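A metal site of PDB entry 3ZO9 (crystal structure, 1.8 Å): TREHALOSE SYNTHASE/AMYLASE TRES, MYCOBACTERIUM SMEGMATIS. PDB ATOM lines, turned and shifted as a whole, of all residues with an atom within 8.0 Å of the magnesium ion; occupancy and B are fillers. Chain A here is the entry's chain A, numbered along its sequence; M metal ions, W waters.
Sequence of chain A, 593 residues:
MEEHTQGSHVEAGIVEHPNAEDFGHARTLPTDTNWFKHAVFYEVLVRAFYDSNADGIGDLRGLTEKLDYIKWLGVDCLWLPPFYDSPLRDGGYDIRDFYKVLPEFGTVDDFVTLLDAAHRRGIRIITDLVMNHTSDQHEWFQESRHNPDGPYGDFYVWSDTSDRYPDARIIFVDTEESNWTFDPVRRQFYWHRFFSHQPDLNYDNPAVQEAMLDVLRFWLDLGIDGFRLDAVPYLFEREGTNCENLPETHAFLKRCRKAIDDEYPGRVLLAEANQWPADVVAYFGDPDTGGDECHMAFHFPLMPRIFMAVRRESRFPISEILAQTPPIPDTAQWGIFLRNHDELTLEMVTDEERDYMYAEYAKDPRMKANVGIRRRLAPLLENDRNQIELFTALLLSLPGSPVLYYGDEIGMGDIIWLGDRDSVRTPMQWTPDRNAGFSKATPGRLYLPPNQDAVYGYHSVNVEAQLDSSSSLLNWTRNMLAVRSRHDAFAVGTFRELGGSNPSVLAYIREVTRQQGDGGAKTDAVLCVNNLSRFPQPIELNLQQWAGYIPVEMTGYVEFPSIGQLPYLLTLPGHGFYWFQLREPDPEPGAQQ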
ATOM      1  N   VAL A  46      12.606  11.658   5.831  1.00  0.00           N
ATOM      2  CA  VAL A  46      11.482  12.269   5.120  1.00  0.00           C
ATOM      3  C   VAL A  46      10.190  11.502   5.352  1.00  0.00           C
ATOM      4  O   VAL A  46       9.154  12.105   5.630  1.00  0.00           O
ATOM      5  CB  VAL A  46      11.789  12.389   3.607  1.00  0.00           C
ATOM      6  CG1 VAL A  46      10.562  12.968   2.858  1.00  0.00           C
ATOM      7  CG2 VAL A  46      13.025  13.271   3.388  1.00  0.00           C
ATOM      8  N   ARG A  47      10.244  10.180   5.280  1.00  0.00           N
ATOM      9  CA  ARG A  47       9.006   9.393   5.391  1.00  0.00           C
ATOM     10  C   ARG A  47       8.325   9.531   6.764  1.00  0.00           C
ATOM     11  O   ARG A  47       7.114   9.332   6.879  1.00  0.00           O
ATOM     12  CB  ARG A  47       9.276   7.906   5.096  1.00  0.00           C
ATOM     13  CG  ARG A  47       9.969   7.159   6.247  1.00  0.00           C
ATOM     14  CD  ARG A  47      10.310   5.719   5.872  1.00  0.00           C
ATOM     15  NE  ARG A  47      11.407   5.625   4.899  1.00  0.00           N
ATOM     16  CZ  ARG A  47      12.230   4.595   4.779  1.00  0.00           C
ATOM     17  NH1 ARG A  47      12.107   3.544   5.577  1.00  0.00           N
ATOM     18  NH2 ARG A  47      13.190   4.590   3.860  1.00  0.00           N
ATOM     19  N   TYR A  50       6.592  14.402   8.678  1.00  0.00           N
ATOM     20  CA  TYR A  50       5.255  14.994   8.575  1.00  0.00           C
ATOM     21  C   TYR A  50       4.625  14.727   7.216  1.00  0.00           C
ATOM     22  O   TYR A  50       5.242  14.964   6.183  1.00  0.00           O
ATOM     23  CB  TYR A  50       5.299  16.488   8.890  1.00  0.00           C
ATOM     24  CG  TYR A  50       3.927  17.114   8.964  1.00  0.00           C
ATOM     25  CD1 TYR A  50       2.989  16.641   9.876  1.00  0.00           C
ATOM     26  CD2 TYR A  50       3.565  18.148   8.131  1.00  0.00           C
ATOM     27  CE1 TYR A  50       1.723  17.190   9.935  1.00  0.00           C
ATOM     28  CE2 TYR A  50       2.305  18.702   8.178  1.00  0.00           C
ATOM     29  CZ  TYR A  50       1.395  18.228   9.088  1.00  0.00           C
ATOM     30  OH  TYR A  50       0.142  18.786   9.140  1.00  0.00           O
ATOM     31  N   ASP A  51       3.422  14.170   7.234  1.00  0.00           N
ATOM     32  CA  ASP A  51       2.662  13.869   6.013  1.00  0.00           C
ATOM     33  C   ASP A  51       1.716  15.019   5.681  1.00  0.00           C
ATOM     34  O   ASP A  51       0.645  15.149   6.281  1.00  0.00           O
ATOM     35  CB  ASP A  51       1.852  12.579   6.222  1.00  0.00           C
ATOM     36  CG  ASP A  51       0.920  12.265   5.067  1.00  0.00           C
ATOM     37  OD1 ASP A  51       1.243  12.650   3.921  1.00  0.00           O
ATOM     38  OD2 ASP A  51      -0.124  11.607   5.296  1.00  0.00           O
ATOM     39  N   SER A  52       2.090  15.871   4.733  1.00  0.00           N
ATOM     40  CA  SER A  52       1.281  17.041   4.420  1.00  0.00           C
ATOM     41  C   SER A  52       0.150  16.733   3.432  1.00  0.00           C
ATOM     42  O   SER A  52      -0.761  17.559   3.245  1.00  0.00           O
ATOM     43  CB  SER A  52       2.146  18.164   3.840  1.00  0.00           C
ATOM     44  OG  SER A  52       2.585  17.816   2.536  1.00  0.00           O
ATOM     45  N   ASN A  53       0.190  15.585   2.767  1.00  0.00           N
ATOM     46  CA  ASN A  53      -0.777  15.311   1.708  1.00  0.00           C
ATOM     47  C   ASN A  53      -1.739  14.159   1.971  1.00  0.00           C
ATOM     48  O   ASN A  53      -2.430  13.691   1.067  1.00  0.00           O
ATOM     49  CB  ASN A  53      -0.088  15.152   0.340  1.00  0.00           C
ATOM     50  CG  ASN A  53       0.948  14.051   0.311  1.00  0.00           C
ATOM     51  OD1 ASN A  53       1.010  13.216   1.212  1.00  0.00           O
ATOM     52  ND2 ASN A  53       1.792  14.044  -0.726  1.00  0.00           N
ATOM     53  N   ALA A  54      -1.782  13.716   3.239  1.00  0.00           N
ATOM     54  CA  ALA A  54      -2.728  12.709   3.693  1.00  0.00           C
ATOM     55  C   ALA A  54      -2.711  11.399   2.918  1.00  0.00           C
ATOM     56  O   ALA A  54      -3.745  10.755   2.758  1.00  0.00           O
ATOM     57  CB  ALA A  54      -4.166  13.298   3.738  1.00  0.00           C
ATOM     58  N   ASP A  55      -1.536  10.977   2.451  1.00  0.00           N
ATOM     59  CA  ASP A  55      -1.396   9.645   1.879  1.00  0.00           C
ATOM     60  C   ASP A  55      -0.786   8.654   2.878  1.00  0.00           C
ATOM     61  O   ASP A  55      -0.603   7.478   2.565  1.00  0.00           O
ATOM     62  CB  ASP A  55      -0.588   9.698   0.579  1.00  0.00           C
ATOM     63  CG  ASP A  55       0.863  10.105   0.800  1.00  0.00           C
ATOM     64  OD1 ASP A  55       1.217  10.522   1.923  1.00  0.00           O
ATOM     65  OD2 ASP A  55       1.641  10.016  -0.175  1.00  0.00           O
ATOM     66  N   GLY A  56      -0.496   9.135   4.082  1.00  0.00           N
ATOM     67  CA  GLY A  56      -0.002   8.278   5.143  1.00  0.00           C
ATOM     68  C   GLY A  56       1.521   8.206   5.191  1.00  0.00           C
ATOM     69  O   GLY A  56       2.087   7.478   6.010  1.00  0.00           O
ATOM     70  N   ILE A  57       2.164   8.956   4.318  1.00  0.00           N
ATOM     71  CA  ILE A  57       3.616   8.894   4.208  1.00  0.00           C
ATOM     72  C   ILE A  57       4.210  10.285   4.308  1.00  0.00           C
ATOM     73  O   ILE A  57       3.715  11.223   3.665  1.00  0.00           O
ATOM     74  CB  ILE A  57       4.032   8.273   2.863  1.00  0.00           C
ATOM     75  CG1 ILE A  57       3.381   6.894   2.681  1.00  0.00           C
ATOM     76  CG2 ILE A  57       5.550   8.166   2.771  1.00  0.00           C
ATOM     77  CD1 ILE A  57       3.669   6.257   1.341  1.00  0.00           C
ATOM     78  N   GLY A  58       5.263  10.437   5.110  1.00  0.00           N
ATOM     79  CA  GLY A  58       5.918  11.738   5.267  1.00  0.00           C
ATOM     80  C   GLY A  58       6.444  12.203   3.920  1.00  0.00           C
ATOM     81  O   GLY A  58       6.773  11.381   3.066  1.00  0.00           O
ATOM     82  N   ASP A  59       6.525  13.520   3.726  1.00  0.00           N
ATOM     83  CA  ASP A  59       6.934  14.046   2.423  1.00  0.00           C
ATOM     84  C   ASP A  59       7.772  15.324   2.548  1.00  0.00           C
ATOM     85  O   ASP A  59       7.924  15.887   3.637  1.00  0.00           O
ATOM     86  CB  ASP A  59       5.690  14.271   1.549  1.00  0.00           C
ATOM     87  CG  ASP A  59       4.506  14.816   2.337  1.00  0.00           C
ATOM     88  OD1 ASP A  59       4.591  16.004   2.715  1.00  0.00           O
ATOM     89  OD2 ASP A  59       3.529  14.056   2.606  1.00  0.00           O
ATOM     90  N   LEU A  60       8.359  15.762   1.421  1.00  0.00           N
ATOM     91  CA  LEU A  60       9.268  16.906   1.469  1.00  0.00           C
ATOM     92  C   LEU A  60       8.529  18.183   1.835  1.00  0.00           C
ATOM     93  O   LEU A  60       9.032  18.983   2.619  1.00  0.00           O
ATOM     94  CB  LEU A  60      10.023  17.078   0.134  1.00  0.00           C
ATOM     95  CG  LEU A  60      11.043  15.993  -0.171  1.00  0.00           C
ATOM     96  CD1 LEU A  60      11.460  16.043  -1.653  1.00  0.00           C
ATOM     97  CD2 LEU A  60      12.275  16.077   0.748  1.00  0.00           C
ATOM     98  N   ARG A  61       7.340  18.372   1.275  1.00  0.00           N
ATOM     99  CA  ARG A  61       6.532  19.534   1.656  1.00  0.00           C
ATOM    100  C   ARG A  61       6.216  19.524   3.154  1.00  0.00           C
ATOM    101  O   ARG A  61       6.225  20.570   3.808  1.00  0.00           O
ATOM    102  CB  ARG A  61       5.243  19.591   0.825  1.00  0.00           C
ATOM    103  CG  ARG A  61       4.325  20.749   1.175  1.00  0.00           C
ATOM    104  CD  ARG A  61       3.363  21.072   0.013  1.00  0.00           C
ATOM    105  NE  ARG A  61       4.064  21.722  -1.098  1.00  0.00           N
ATOM    106  CZ  ARG A  61       3.484  22.220  -2.180  1.00  0.00           C
ATOM    107  NH1 ARG A  61       2.166  22.155  -2.338  1.00  0.00           N
ATOM    108  NH2 ARG A  61       4.220  22.800  -3.132  1.00  0.00           N
ATOM    109  N   GLY A  62       5.951  18.342   3.701  1.00  0.00           N
ATOM    110  CA  GLY A  62       5.672  18.211   5.125  1.00  0.00           C
ATOM    111  C   GLY A  62       6.869  18.582   5.968  1.00  0.00           C
ATOM    112  O   GLY A  62       6.744  19.317   6.961  1.00  0.00           O
ATOM    113  N   GLU A 104       6.585   9.284  -3.819  1.00  0.00           N
ATOM    114  CA  GLU A 104       5.698   9.581  -2.694  1.00  0.00           C
ATOM    115  C   GLU A 104       6.216  10.702  -1.797  1.00  0.00           C
ATOM    116  O   GLU A 104       5.458  11.263  -1.004  1.00  0.00           O
ATOM    117  CB  GLU A 104       5.356   8.321  -1.881  1.00  0.00           C
ATOM    118  CG  GLU A 104       6.537   7.609  -1.268  1.00  0.00           C
ATOM    119  CD  GLU A 104       6.357   6.106  -1.247  1.00  0.00           C
ATOM    120  OE1 GLU A 104       5.931   5.555  -2.296  1.00  0.00           O
ATOM    121  OE2 GLU A 104       6.657   5.474  -0.213  1.00  0.00           O
ATOM    122  N   PHE A 105       7.495  11.064  -1.945  1.00  0.00           N
ATOM    123  CA  PHE A 105       8.056  12.204  -1.219  1.00  0.00           C
ATOM    124  C   PHE A 105       7.887  13.547  -1.937  1.00  0.00           C
ATOM    125  O   PHE A 105       7.965  14.601  -1.311  1.00  0.00           O
ATOM    126  CB  PHE A 105       9.554  11.999  -0.957  1.00  0.00           C
ATOM    127  CG  PHE A 105       9.857  10.821  -0.063  1.00  0.00           C
ATOM    128  CD1 PHE A 105       8.902  10.324   0.815  1.00  0.00           C
ATOM    129  CD2 PHE A 105      11.120  10.251  -0.081  1.00  0.00           C
ATOM    130  CE1 PHE A 105       9.201   9.261   1.648  1.00  0.00           C
ATOM    131  CE2 PHE A 105      11.425   9.185   0.744  1.00  0.00           C
ATOM    132  CZ  PHE A 105      10.462   8.683   1.618  1.00  0.00           C
ATOM    133  N   GLY A 106       7.673  13.501  -3.241  1.00  0.00           N
ATOM    134  CA  GLY A 106       7.590  14.718  -4.043  1.00  0.00           C
ATOM    135  C   GLY A 106       8.543  14.635  -5.217  1.00  0.00           C
ATOM    136  O   GLY A 106       8.863  13.539  -5.674  1.00  0.00           O
ATOM    137  N   PHE A 438       0.779  13.193  13.003  1.00  0.00           N
ATOM    138  CA  PHE A 438       1.708  13.044  11.876  1.00  0.00           C
ATOM    139  C   PHE A 438       0.980  13.087  10.535  1.00  0.00           C
ATOM    140  O   PHE A 438       1.541  13.504   9.520  1.00  0.00           O
ATOM    141  CB  PHE A 438       2.476  11.729  12.035  1.00  0.00           C
ATOM    142  CG  PHE A 438       3.038  11.173  10.754  1.00  0.00           C
ATOM    143  CD1 PHE A 438       4.259  11.629  10.252  1.00  0.00           C
ATOM    144  CD2 PHE A 438       2.361  10.159  10.080  1.00  0.00           C
ATOM    145  CE1 PHE A 438       4.772  11.113   9.069  1.00  0.00           C
ATOM    146  CE2 PHE A 438       2.874   9.618   8.895  1.00  0.00           C
ATOM    147  CZ  PHE A 438       4.079  10.091   8.384  1.00  0.00           C
ATOM    148  N   SER A 439      -0.284  12.661  10.518  1.00  0.00           N
ATOM    149  CA  SER A 439      -1.032  12.548   9.270  1.00  0.00           C
ATOM    150  C   SER A 439      -2.526  12.670   9.487  1.00  0.00           C
ATOM    151  O   SER A 439      -3.018  12.339  10.567  1.00  0.00           O
ATOM    152  CB  SER A 439      -0.740  11.168   8.650  1.00  0.00           C
ATOM    153  OG  SER A 439      -1.457  10.981   7.433  1.00  0.00           O
ATOM    154  N   ALA A 441      -4.397  10.925   7.322  1.00  0.00           N
ATOM    155  CA  ALA A 441      -4.860   9.691   6.662  1.00  0.00           C
ATOM    156  C   ALA A 441      -5.490   8.752   7.683  1.00  0.00           C
ATOM    157  O   ALA A 441      -5.384   8.971   8.893  1.00  0.00           O
ATOM    158  CB  ALA A 441      -3.713   9.007   5.922  1.00  0.00           C
HETATM  159 MG    MG M   1       2.519  12.270   2.356  1.00  0.00          MG
HETATM  160  O   HOH W   1       3.581  11.704   0.594  1.00  0.00           O
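Water W1 lies within hydrogen-bond range of the backbone carbonyl oxygen (O) of Glu 104 (2.5 Å), the side-chain carboxylate (OD2) of Asp 55 (2.7 Å) and the side-chain amide nitrogen (ND2) of Asn 53 (3.2 Å).
The backbone NH (N) of Asp 59 sits at hydrogen-bond distance from the backbone carbonyl oxygen (O) of Tyr 50, at 3.1 Å.
The side-chain carboxylate (OD2) of Asp 51 sits close to the backbone NH (N) of Ala 54.
N of Gly 56 sits at hydrogen-bond distance from OD2 of Asp 51 (2.8 Å).
N of Asp 51 sits at hydrogen-bond distance from O of Phe 438 (3.0 Å).
The side-chain hydroxyl (OG) of Ser 52 sits at hydrogen-bond distance from the side-chain carboxylate (OD1) of Asp 59 (2.7 Å).
The side-chain carboxylate (OD2) of Asp 51 sits at hydrogen-bond distance from the side-chain hydroxyl (OG) of Ser 439.
The side-chain carboxylate of Asp 59 sits at hydrogen-bond distance from the backbone NH of Gly 62, at 2.9 Å.
The magnesium ion is bound by the side-chain carboxylate of Asp 51 (2.1 Å), the backbone carbonyl oxygen of Ile 57 (2.1 Å), the side-chain carboxylate of Asp 59 (2.1 Å), the side-chain amide oxygen of Asn 53 (2.1 Å), water W1 (2.1 Å) and the side-chain carboxylate of Asp 55 (2.2 Å).
Of the 21 residues printed, 5 come within 4 Å of the magnesium ion.
The nearest printed residue that does not touch the magnesium ion is Gly 58 (4.2 Å).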
